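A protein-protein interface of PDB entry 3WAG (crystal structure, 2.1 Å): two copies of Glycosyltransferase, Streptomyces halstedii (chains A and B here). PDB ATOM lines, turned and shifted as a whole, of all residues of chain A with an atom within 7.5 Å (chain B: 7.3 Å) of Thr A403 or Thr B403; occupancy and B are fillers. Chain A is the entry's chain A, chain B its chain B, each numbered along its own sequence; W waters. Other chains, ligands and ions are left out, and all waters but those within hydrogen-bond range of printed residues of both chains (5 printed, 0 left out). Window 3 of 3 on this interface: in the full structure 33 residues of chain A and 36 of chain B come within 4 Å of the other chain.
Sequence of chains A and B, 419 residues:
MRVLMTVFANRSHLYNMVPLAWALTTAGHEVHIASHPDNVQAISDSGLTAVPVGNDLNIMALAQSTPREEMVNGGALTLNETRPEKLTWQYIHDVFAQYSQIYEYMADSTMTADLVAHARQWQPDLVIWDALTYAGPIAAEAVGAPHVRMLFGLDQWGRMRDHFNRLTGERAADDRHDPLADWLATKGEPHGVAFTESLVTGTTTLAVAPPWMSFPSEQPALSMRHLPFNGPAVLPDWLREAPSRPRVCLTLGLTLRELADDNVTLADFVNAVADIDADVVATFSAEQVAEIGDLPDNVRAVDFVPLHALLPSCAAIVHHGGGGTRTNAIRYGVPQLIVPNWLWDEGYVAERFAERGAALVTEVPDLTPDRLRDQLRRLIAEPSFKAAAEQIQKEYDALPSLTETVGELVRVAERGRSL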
ATOM      1  N   LEU A  20       5.851  10.495  11.921  1.00  0.00           N
ATOM      2  CA  LEU A  20       7.134  10.399  11.245  1.00  0.00           C
ATOM      3  C   LEU A  20       7.475   8.955  10.747  1.00  0.00           C
ATOM      4  O   LEU A  20       7.791   8.747   9.557  1.00  0.00           O
ATOM      5  CB  LEU A  20       8.237  10.914  12.152  1.00  0.00           C
ATOM      6  CG  LEU A  20       9.539  11.099  11.404  1.00  0.00           C
ATOM      7  CD1 LEU A  20       9.283  12.102  10.273  1.00  0.00           C
ATOM      8  CD2 LEU A  20      10.592  11.551  12.377  1.00  0.00           C
ATOM      9  N   ALA A  23       5.490   8.429   7.786  1.00  0.00           N
ATOM     10  CA  ALA A  23       5.978   9.257   6.649  1.00  0.00           C
ATOM     11  C   ALA A  23       7.151   8.540   6.039  1.00  0.00           C
ATOM     12  O   ALA A  23       7.241   8.409   4.828  1.00  0.00           O
ATOM     13  CB  ALA A  23       6.405  10.631   7.141  1.00  0.00           C
ATOM     14  N   THR A  26       5.594   5.147   4.157  1.00  0.00           N
ATOM     15  CA  THR A  26       4.966   5.378   2.871  1.00  0.00           C
ATOM     16  C   THR A  26       5.906   5.976   1.803  1.00  0.00           C
ATOM     17  O   THR A  26       5.595   5.871   0.637  1.00  0.00           O
ATOM     18  CB  THR A  26       3.631   6.142   2.985  1.00  0.00           C
ATOM     19  OG1 THR A  26       3.884   7.458   3.468  1.00  0.00           O
ATOM     20  CG2 THR A  26       2.731   5.434   3.975  1.00  0.00           C
ATOM     21  N   ALA A  27       7.015   6.606   2.190  1.00  0.00           N
ATOM     22  CA  ALA A  27       8.059   7.038   1.234  1.00  0.00           C
ATOM     23  C   ALA A  27       8.879   5.852   0.776  1.00  0.00           C
ATOM     24  O   ALA A  27       9.760   6.005  -0.036  1.00  0.00           O
ATOM     25  CB  ALA A  27       8.984   8.083   1.870  1.00  0.00           C
ATOM     26  N   GLY A  28       8.630   4.674   1.362  1.00  0.00           N
ATOM     27  CA  GLY A  28       9.247   3.434   0.909  1.00  0.00           C
ATOM     28  C   GLY A  28      10.380   2.952   1.780  1.00  0.00           C
ATOM     29  O   GLY A  28      10.975   1.938   1.484  1.00  0.00           O
ATOM     30  N   ARG A 225       6.034  20.700  10.938  1.00  0.00           N
ATOM     31  CA  ARG A 225       4.649  20.868  11.281  1.00  0.00           C
ATOM     32  C   ARG A 225       4.202  19.532  11.955  1.00  0.00           C
ATOM     33  O   ARG A 225       3.780  18.595  11.278  1.00  0.00           O
ATOM     34  CB  ARG A 225       3.836  21.104  10.018  1.00  0.00           C
ATOM     35  CG  ARG A 225       2.339  21.144  10.239  1.00  0.00           C
ATOM     36  CD  ARG A 225       1.580  21.446   8.947  1.00  0.00           C
ATOM     37  NE  ARG A 225       1.711  20.405   7.915  1.00  0.00           N
ATOM     38  CZ  ARG A 225       1.351  20.566   6.634  1.00  0.00           C
ATOM     39  NH1 ARG A 225       0.894  21.744   6.200  1.00  0.00           N
ATOM     40  NH2 ARG A 225       1.499  19.580   5.746  1.00  0.00           N
ATOM     41  N   PRO A 400       7.411  23.033   7.775  1.00  0.00           N
ATOM     42  CA  PRO A 400       7.637  21.957   6.833  1.00  0.00           C
ATOM     43  C   PRO A 400       6.699  20.719   7.060  1.00  0.00           C
ATOM     44  O   PRO A 400       6.587  20.186   8.193  1.00  0.00           O
ATOM     45  CB  PRO A 400       9.087  21.573   7.094  1.00  0.00           C
ATOM     46  CG  PRO A 400       9.707  22.768   7.772  1.00  0.00           C
ATOM     47  CD  PRO A 400       8.627  23.418   8.521  1.00  0.00           C
ATOM     48  N   SER A 401       6.030  20.289   5.988  1.00  0.00           N
ATOM     49  CA  SER A 401       5.192  19.100   5.996  1.00  0.00           C
ATOM     50  C   SER A 401       5.991  17.854   6.387  1.00  0.00           C
ATOM     51  O   SER A 401       7.230  17.874   6.419  1.00  0.00           O
ATOM     52  CB  SER A 401       4.575  18.922   4.603  1.00  0.00           C
ATOM     53  OG  SER A 401       5.565  18.428   3.774  1.00  0.00           O
ATOM     54  N   LEU A 402       5.313  16.741   6.694  1.00  0.00           N
ATOM     55  CA  LEU A 402       6.129  15.529   7.003  1.00  0.00           C
ATOM     56  C   LEU A 402       6.922  15.068   5.760  1.00  0.00           C
ATOM     57  O   LEU A 402       8.034  14.538   5.861  1.00  0.00           O
ATOM     58  CB  LEU A 402       5.321  14.404   7.672  1.00  0.00           C
ATOM     59  CG  LEU A 402       5.401  14.594   9.193  1.00  0.00           C
ATOM     60  CD1 LEU A 402       4.463  15.685   9.716  1.00  0.00           C
ATOM     61  CD2 LEU A 402       5.130  13.304   9.928  1.00  0.00           C
ATOM     62  N   THR A 403       6.376  15.294   4.586  1.00  0.00           N
ATOM     63  CA  THR A 403       7.115  14.854   3.376  1.00  0.00           C
ATOM     64  C   THR A 403       8.432  15.668   3.256  1.00  0.00           C
ATOM     65  O   THR A 403       9.518  15.097   3.029  1.00  0.00           O
ATOM     66  CB  THR A 403       6.259  15.088   2.128  1.00  0.00           C
ATOM     67  OG1 THR A 403       4.933  14.595   2.354  1.00  0.00           O
ATOM     68  CG2 THR A 403       6.818  14.398   0.989  1.00  0.00           C
ATOM     69  N   GLU A 404       8.360  16.999   3.430  1.00  0.00           N
ATOM     70  CA  GLU A 404       9.615  17.774   3.490  1.00  0.00           C
ATOM     71  C   GLU A 404      10.532  17.163   4.476  1.00  0.00           C
ATOM     72  O   GLU A 404      11.672  16.967   4.208  1.00  0.00           O
ATOM     73  CB  GLU A 404       9.368  19.240   3.929  1.00  0.00           C
ATOM     74  CG  GLU A 404       8.895  20.115   2.791  1.00  0.00           C
ATOM     75  CD  GLU A 404       8.442  21.470   3.266  1.00  0.00           C
ATOM     76  OE1 GLU A 404       9.241  22.189   3.913  1.00  0.00           O
ATOM     77  OE2 GLU A 404       7.266  21.773   3.028  1.00  0.00           O
ATOM     78  N   THR A 405      10.029  16.853   5.667  1.00  0.00           N
ATOM     79  CA  THR A 405      10.931  16.371   6.734  1.00  0.00           C
ATOM     80  C   THR A 405      11.643  15.074   6.351  1.00  0.00           C
ATOM     81  O   THR A 405      12.870  14.886   6.620  1.00  0.00           O
ATOM     82  CB  THR A 405      10.154  16.215   8.084  1.00  0.00           C
ATOM     83  OG1 THR A 405       9.404  17.385   8.335  1.00  0.00           O
ATOM     84  CG2 THR A 405      11.094  15.925   9.274  1.00  0.00           C
ATOM     85  N   VAL A 406      10.887  14.168   5.723  1.00  0.00           N
ATOM     86  CA  VAL A 406      11.490  12.910   5.140  1.00  0.00           C
ATOM     87  C   VAL A 406      12.691  13.167   4.186  1.00  0.00           C
ATOM     88  O   VAL A 406      13.748  12.532   4.299  1.00  0.00           O
ATOM     89  CB  VAL A 406      10.393  11.976   4.487  1.00  0.00           C
ATOM     90  CG1 VAL A 406      11.029  10.805   3.725  1.00  0.00           C
ATOM     91  CG2 VAL A 406       9.439  11.449   5.586  1.00  0.00           C
ATOM     92  N   GLY A 407      12.535  14.150   3.292  1.00  0.00           N
ATOM     93  CA  GLY A 407      13.654  14.642   2.395  1.00  0.00           C
ATOM     94  C   GLY A 407      14.817  15.141   3.234  1.00  0.00           C
ATOM     95  O   GLY A 407      15.939  14.739   3.020  1.00  0.00           O
ATOM     96  N   GLU A 408      14.546  15.925   4.272  1.00  0.00           N
ATOM     97  CA  GLU A 408      15.661  16.322   5.151  1.00  0.00           C
ATOM     98  C   GLU A 408      16.343  15.100   5.741  1.00  0.00           C
ATOM     99  O   GLU A 408      17.596  15.001   5.794  1.00  0.00           O
ATOM    100  CB  GLU A 408      15.181  17.226   6.268  1.00  0.00           C
ATOM    101  CG  GLU A 408      14.498  18.475   5.826  1.00  0.00           C
ATOM    102  CD  GLU A 408      15.502  19.551   5.393  1.00  0.00           C
ATOM    103  OE1 GLU A 408      16.740  19.318   5.452  1.00  0.00           O
ATOM    104  OE2 GLU A 408      15.037  20.642   5.010  1.00  0.00           O
ATOM    105  N   LEU A 409      15.542  14.119   6.179  1.00  0.00           N
ATOM    106  CA  LEU A 409      16.193  12.981   6.838  1.00  0.00           C
ATOM    107  C   LEU A 409      16.923  12.106   5.822  1.00  0.00           C
ATOM    108  O   LEU A 409      18.026  11.617   6.116  1.00  0.00           O
ATOM    109  CB  LEU A 409      15.198  12.199   7.705  1.00  0.00           C
ATOM    110  CG  LEU A 409      14.413  13.018   8.733  1.00  0.00           C
ATOM    111  CD1 LEU A 409      13.185  12.239   9.154  1.00  0.00           C
ATOM    112  CD2 LEU A 409      15.266  13.339   9.948  1.00  0.00           C
ATOM    113  N   VAL A 410      16.340  11.904   4.626  1.00  0.00           N
ATOM    114  CA  VAL A 410      17.159  11.355   3.509  1.00  0.00           C
ATOM    115  C   VAL A 410      18.504  12.093   3.356  1.00  0.00           C
ATOM    116  O   VAL A 410      19.535  11.430   3.322  1.00  0.00           O
ATOM    117  CB  VAL A 410      16.435  11.319   2.138  1.00  0.00           C
ATOM    118  CG1 VAL A 410      17.372  10.711   1.089  1.00  0.00           C
ATOM    119  CG2 VAL A 410      15.201  10.465   2.214  1.00  0.00           C
ATOM    120  N   ARG A 411      18.524  13.444   3.322  1.00  0.00           N
ATOM    121  CA  ARG A 411      19.842  14.173   3.193  1.00  0.00           C
ATOM    122  C   ARG A 411      20.752  13.859   4.368  1.00  0.00           C
ATOM    123  O   ARG A 411      21.959  13.600   4.181  1.00  0.00           O
ATOM    124  CB  ARG A 411      19.745  15.716   3.068  1.00  0.00           C
ATOM    125  CG  ARG A 411      18.450  16.228   2.497  1.00  0.00           C
ATOM    126  CD  ARG A 411      18.532  17.581   1.818  1.00  0.00           C
ATOM    127  NE  ARG A 411      17.552  17.576   0.731  1.00  0.00           N
ATOM    128  CZ  ARG A 411      16.256  17.873   0.858  1.00  0.00           C
ATOM    129  NH1 ARG A 411      15.750  18.243   2.032  1.00  0.00           N
ATOM    130  NH2 ARG A 411      15.456  17.801  -0.204  1.00  0.00           N
ATOM    131  N   LEU B  20      -2.018   3.976   1.669  1.00  0.00           N
ATOM    132  CA  LEU B  20      -2.590   5.224   1.084  1.00  0.00           C
ATOM    133  C   LEU B  20      -3.253   6.177   2.159  1.00  0.00           C
ATOM    134  O   LEU B  20      -3.094   7.408   2.138  1.00  0.00           O
ATOM    135  CB  LEU B  20      -3.567   4.903  -0.042  1.00  0.00           C
ATOM    136  CG  LEU B  20      -4.212   6.125  -0.722  1.00  0.00           C
ATOM    137  CD1 LEU B  20      -3.200   6.880  -1.542  1.00  0.00           C
ATOM    138  CD2 LEU B  20      -5.421   5.809  -1.575  1.00  0.00           C
ATOM    139  N   ALA B  23      -0.312   7.836   3.882  1.00  0.00           N
ATOM    140  CA  ALA B  23       0.384   8.834   2.979  1.00  0.00           C
ATOM    141  C   ALA B  23      -0.368  10.154   2.999  1.00  0.00           C
ATOM    142  O   ALA B  23       0.233  11.219   3.170  1.00  0.00           O
ATOM    143  CB  ALA B  23       0.499   8.333   1.540  1.00  0.00           C
ATOM    144  N   LEU B  24      -1.675  10.060   2.821  1.00  0.00           N
ATOM    145  CA  LEU B  24      -2.595  11.168   2.963  1.00  0.00           C
ATOM    146  C   LEU B  24      -2.571  11.795   4.366  1.00  0.00           C
ATOM    147  O   LEU B  24      -2.595  13.041   4.503  1.00  0.00           O
ATOM    148  CB  LEU B  24      -4.013  10.715   2.629  1.00  0.00           C
ATOM    149  CG  LEU B  24      -4.405  10.426   1.164  1.00  0.00           C
ATOM    150  CD1 LEU B  24      -5.731   9.649   1.182  1.00  0.00           C
ATOM    151  CD2 LEU B  24      -4.550  11.733   0.307  1.00  0.00           C
ATOM    152  N   THR B  26      -0.098  11.836   6.515  1.00  0.00           N
ATOM    153  CA  THR B  26       1.119  12.557   6.815  1.00  0.00           C
ATOM    154  C   THR B  26       1.441  13.700   5.794  1.00  0.00           C
ATOM    155  O   THR B  26       2.352  14.467   6.023  1.00  0.00           O
ATOM    156  CB  THR B  26       2.288  11.617   6.936  1.00  0.00           C
ATOM    157  OG1 THR B  26       2.458  10.942   5.685  1.00  0.00           O
ATOM    158  CG2 THR B  26       2.037  10.564   8.153  1.00  0.00           C
ATOM    159  N   ALA B  27       0.727  13.738   4.678  1.00  0.00           N
ATOM    160  CA  ALA B  27       0.620  14.919   3.820  1.00  0.00           C
ATOM    161  C   ALA B  27      -0.282  15.966   4.471  1.00  0.00           C
ATOM    162  O   ALA B  27      -0.383  17.069   3.947  1.00  0.00           O
ATOM    163  CB  ALA B  27       0.029  14.550   2.464  1.00  0.00           C
ATOM    164  N   GLY B  28      -1.018  15.611   5.534  1.00  0.00           N
ATOM    165  CA  GLY B  28      -1.731  16.639   6.343  1.00  0.00           C
ATOM    166  C   GLY B  28      -3.233  16.686   6.275  1.00  0.00           C
ATOM    167  O   GLY B  28      -3.841  17.564   6.889  1.00  0.00           O
ATOM    168  N   ARG B 225       2.993   2.809  -7.043  1.00  0.00           N
ATOM    169  CA  ARG B 225       3.867   1.809  -6.477  1.00  0.00           C
ATOM    170  C   ARG B 225       3.181   1.323  -5.154  1.00  0.00           C
ATOM    171  O   ARG B 225       3.455   1.842  -4.058  1.00  0.00           O
ATOM    172  CB  ARG B 225       5.259   2.431  -6.219  1.00  0.00           C
ATOM    173  CG  ARG B 225       6.301   1.465  -5.671  1.00  0.00           C
ATOM    174  CD  ARG B 225       7.656   2.101  -5.399  1.00  0.00           C
ATOM    175  NE  ARG B 225       7.529   3.216  -4.436  1.00  0.00           N
ATOM    176  CZ  ARG B 225       8.337   4.267  -4.369  1.00  0.00           C
ATOM    177  NH1 ARG B 225       9.333   4.381  -5.232  1.00  0.00           N
ATOM    178  NH2 ARG B 225       8.147   5.214  -3.451  1.00  0.00           N
ATOM    179  N   PRO B 400       4.459   5.478  -9.760  1.00  0.00           N
ATOM    180  CA  PRO B 400       4.378   6.640  -8.915  1.00  0.00           C
ATOM    181  C   PRO B 400       4.363   6.320  -7.388  1.00  0.00           C
ATOM    182  O   PRO B 400       3.730   5.373  -6.931  1.00  0.00           O
ATOM    183  CB  PRO B 400       3.080   7.297  -9.365  1.00  0.00           C
ATOM    184  CG  PRO B 400       2.802   6.764 -10.748  1.00  0.00           C
ATOM    185  CD  PRO B 400       3.274   5.348 -10.638  1.00  0.00           C
ATOM    186  N   SER B 401       5.069   7.122  -6.622  1.00  0.00           N
ATOM    187  CA  SER B 401       5.255   6.912  -5.231  1.00  0.00           C
ATOM    188  C   SER B 401       3.943   7.255  -4.548  1.00  0.00           C
ATOM    189  O   SER B 401       3.006   7.767  -5.168  1.00  0.00           O
ATOM    190  CB  SER B 401       6.389   7.831  -4.751  1.00  0.00           C
ATOM    191  OG  SER B 401       5.941   9.158  -4.615  1.00  0.00           O
ATOM    192  N   LEU B 402       3.823   6.961  -3.260  1.00  0.00           N
ATOM    193  CA  LEU B 402       2.554   7.306  -2.608  1.00  0.00           C
ATOM    194  C   LEU B 402       2.352   8.857  -2.479  1.00  0.00           C
ATOM    195  O   LEU B 402       1.233   9.329  -2.607  1.00  0.00           O
ATOM    196  CB  LEU B 402       2.430   6.579  -1.239  1.00  0.00           C
ATOM    197  CG  LEU B 402       1.625   5.273  -1.077  1.00  0.00           C
ATOM    198  CD1 LEU B 402       1.782   4.376  -2.256  1.00  0.00           C
ATOM    199  CD2 LEU B 402       2.197   4.493   0.077  1.00  0.00           C
ATOM    200  N   THR B 403       3.405   9.592  -2.138  1.00  0.00           N
ATOM    201  CA  THR B 403       3.436  11.084  -2.115  1.00  0.00           C
ATOM    202  C   THR B 403       2.900  11.686  -3.438  1.00  0.00           C
ATOM    203  O   THR B 403       1.888  12.403  -3.465  1.00  0.00           O
ATOM    204  CB  THR B 403       4.870  11.561  -1.952  1.00  0.00           C
ATOM    205  OG1 THR B 403       5.399  10.992  -0.761  1.00  0.00           O
ATOM    206  CG2 THR B 403       4.966  13.114  -1.833  1.00  0.00           C
ATOM    207  N   GLU B 404       3.521  11.268  -4.525  1.00  0.00           N
ATOM    208  CA  GLU B 404       2.997  11.478  -5.878  1.00  0.00           C
ATOM    209  C   GLU B 404       1.524  11.104  -6.052  1.00  0.00           C
ATOM    210  O   GLU B 404       0.758  11.858  -6.679  1.00  0.00           O
ATOM    211  CB  GLU B 404       3.817  10.639  -6.843  1.00  0.00           C
ATOM    212  CG  GLU B 404       4.711  11.374  -7.797  1.00  0.00           C
ATOM    213  CD  GLU B 404       5.383  10.388  -8.722  1.00  0.00           C
ATOM    214  OE1 GLU B 404       4.932  10.249  -9.920  1.00  0.00           O
ATOM    215  OE2 GLU B 404       6.310   9.723  -8.201  1.00  0.00           O
ATOM    216  N   THR B 405       1.105   9.950  -5.502  1.00  0.00           N
ATOM    217  CA  THR B 405      -0.297   9.531  -5.643  1.00  0.00           C
ATOM    218  C   THR B 405      -1.227  10.441  -4.865  1.00  0.00           C
ATOM    219  O   THR B 405      -2.364  10.731  -5.323  1.00  0.00           O
ATOM    220  CB  THR B 405      -0.525   8.043  -5.222  1.00  0.00           C
ATOM    221  OG1 THR B 405       0.249   7.178  -6.070  1.00  0.00           O
ATOM    222  CG2 THR B 405      -2.005   7.661  -5.370  1.00  0.00           C
ATOM    223  N   VAL B 406      -0.772  10.890  -3.692  1.00  0.00           N
ATOM    224  CA  VAL B 406      -1.531  11.892  -2.916  1.00  0.00           C
ATOM    225  C   VAL B 406      -1.702  13.201  -3.758  1.00  0.00           C
ATOM    226  O   VAL B 406      -2.776  13.779  -3.785  1.00  0.00           O
ATOM    227  CB  VAL B 406      -0.805  12.242  -1.586  1.00  0.00           C
ATOM    228  CG1 VAL B 406      -1.339  13.588  -1.014  1.00  0.00           C
ATOM    229  CG2 VAL B 406      -0.953  11.075  -0.587  1.00  0.00           C
ATOM    230  N   GLY B 407      -0.646  13.648  -4.443  1.00  0.00           N
ATOM    231  CA  GLY B 407      -0.747  14.841  -5.315  1.00  0.00           C
ATOM    232  C   GLY B 407      -1.769  14.596  -6.416  1.00  0.00           C
ATOM    233  O   GLY B 407      -2.696  15.360  -6.592  1.00  0.00           O
ATOM    234  N   GLU B 408      -1.628  13.462  -7.095  1.00  0.00           N
ATOM    235  CA  GLU B 408      -2.620  13.028  -8.031  1.00  0.00           C
ATOM    236  C   GLU B 408      -3.936  13.110  -7.398  1.00  0.00           C
ATOM    237  O   GLU B 408      -4.880  13.619  -8.004  1.00  0.00           O
ATOM    238  CB  GLU B 408      -2.322  11.606  -8.599  1.00  0.00           C
ATOM    239  CG  GLU B 408      -1.591  11.591  -9.929  1.00  0.00           C
ATOM    240  CD  GLU B 408      -2.063  12.715 -10.842  1.00  0.00           C
ATOM    241  OE1 GLU B 408      -3.182  12.640 -11.407  1.00  0.00           O
ATOM    242  OE2 GLU B 408      -1.336  13.726 -10.933  1.00  0.00           O
ATOM    243  N   LEU B 409      -4.055  12.649  -6.140  1.00  0.00           N
ATOM    244  CA  LEU B 409      -5.414  12.620  -5.552  1.00  0.00           C
ATOM    245  C   LEU B 409      -5.891  14.032  -5.091  1.00  0.00           C
ATOM    246  O   LEU B 409      -7.095  14.333  -5.054  1.00  0.00           O
ATOM    247  CB  LEU B 409      -5.491  11.589  -4.385  1.00  0.00           C
ATOM    248  CG  LEU B 409      -5.545  10.067  -4.664  1.00  0.00           C
ATOM    249  CD1 LEU B 409      -5.152   9.300  -3.395  1.00  0.00           C
ATOM    250  CD2 LEU B 409      -6.906   9.595  -5.138  1.00  0.00           C
ATOM    251  N   ARG B 411      -5.289  16.456  -6.945  1.00  0.00           N
ATOM    252  CA  ARG B 411      -5.794  16.955  -8.259  1.00  0.00           C
ATOM    253  C   ARG B 411      -7.201  16.521  -8.590  1.00  0.00           C
ATOM    254  O   ARG B 411      -8.007  17.333  -9.106  1.00  0.00           O
ATOM    255  CB  ARG B 411      -4.838  16.657  -9.403  1.00  0.00           C
ATOM    256  CG  ARG B 411      -3.663  17.610  -9.383  1.00  0.00           C
ATOM    257  CD  ARG B 411      -2.500  17.166 -10.251  1.00  0.00           C
ATOM    258  NE  ARG B 411      -1.273  17.508  -9.547  1.00  0.00           N
ATOM    259  CZ  ARG B 411      -0.322  16.646  -9.195  1.00  0.00           C
ATOM    260  NH1 ARG B 411      -0.401  15.362  -9.515  1.00  0.00           N
ATOM    261  NH2 ARG B 411       0.734  17.090  -8.537  1.00  0.00           N
HETATM  262  O   HOH W   1       2.863   8.300   5.880  1.00  0.00           O
HETATM  263  O   HOH W   2       4.639  12.152   4.072  1.00  0.00           O
HETATM  264  O   HOH W   3       2.645  17.163   6.988  1.00  0.00           O
HETATM  265  O   HOH W   4       5.992   5.224  -2.040  1.00  0.00           O
HETATM  266  O   HOH W   5       5.849   8.501  -1.148  1.00  0.00           O
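N of Arg B225 sits at hydrogen-bond distance from O of Pro B400 (2.7 Å).
N of Arg A225 sits at hydrogen-bond distance from O of Pro A400 (2.8 Å).
The backbone NH of Thr A403 sits close to the side-chain hydroxyl of Ser A401 (3.3 Å).
The side-chain hydroxyl of Thr B26 lies within hydrogen-bond range of the backbone carbonyl oxygen of Ala B23 (3.4 Å).
Among the printed residues, merely in contact across the chains: Thr A26 with Ala B23, Thr A26 with Leu B402, Ala A27 with Arg B225, Arg A225 with Ala B27, Leu A402 with Thr B26 and Thr A403 with Thr B403.
Thr A403 touches just one residue of chain B: Thr B403.
Of the printed residues of chain B, Arg A225 touches Ala B27.
Printed residues of chain B within 4 Å of Thr A26: Ala B23 and Leu B402.
Printed residues of chain A within 4 Å of Arg B225: Ala A27.
Of the printed residues of chain A, Leu B402 touches Thr A26.
The nearest residue of chain A that does not touch Thr B403 is Thr A26 (5.1 Å).
The nearest printed residue of chain A that does not touch Thr B26 is Ala A23 (4.02 Å).
Printed residues of chain B that touch a printed residue of chain A: Ala B23, Thr B26, Ala B27, Arg B225, Leu B402 and Thr B403.
Printed residues of chain A that touch a printed residue of chain B: Thr A26, Ala A27, Arg A225, Leu A402 and Thr A403.
Among the printed residues, 6 pairs touch across the chains.
Thr A26 touches Ala B23, but with the chains exchanged Ala A23 does not touch Thr B26 (4.02 Å).
Thr A26 touches Leu B402, and with the chains exchanged Leu A402 touches Thr B26.
Ala A27 touches Arg B225, and with the chains exchanged Arg A225 touches Ala B27.
Thr A403 touches its own counterpart, Thr B403.
Positions printed for both chains: 20, 23, 26, 27, 28, 225, 400, 401, 402, 403, 404, 405, 406, 407, 408, 409 and 411.
Of the 6 pairs that touch across the chains among the printed residues, 5 have their exchanged pair printed and touching as well.
Water W5 lies within hydrogen-bond range of the side-chain hydroxyl of Thr B403, the backbone carbonyl oxygen of Thr A26 and the backbone NH of Leu B402.
Water W4 lies within hydrogen-bond range of the guanidinium group of Arg B225 (2.6 Å), the backbone carbonyl oxygen of Thr A26 (2.8 Å) and the backbone NH of Leu B402 (3.0 Å).
Water W1 lies within hydrogen-bond range of OG1 of Thr B26, OG1 of Thr A26 and N of Ala A23.
Water W3 lies within hydrogen-bond range of N of Leu A402, O of Thr B26 and NH2 of Arg A225.
Water W2 bridges OG1 of Thr B26 (3.0 Å) and OG1 of Thr A403 (3.0 Å).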
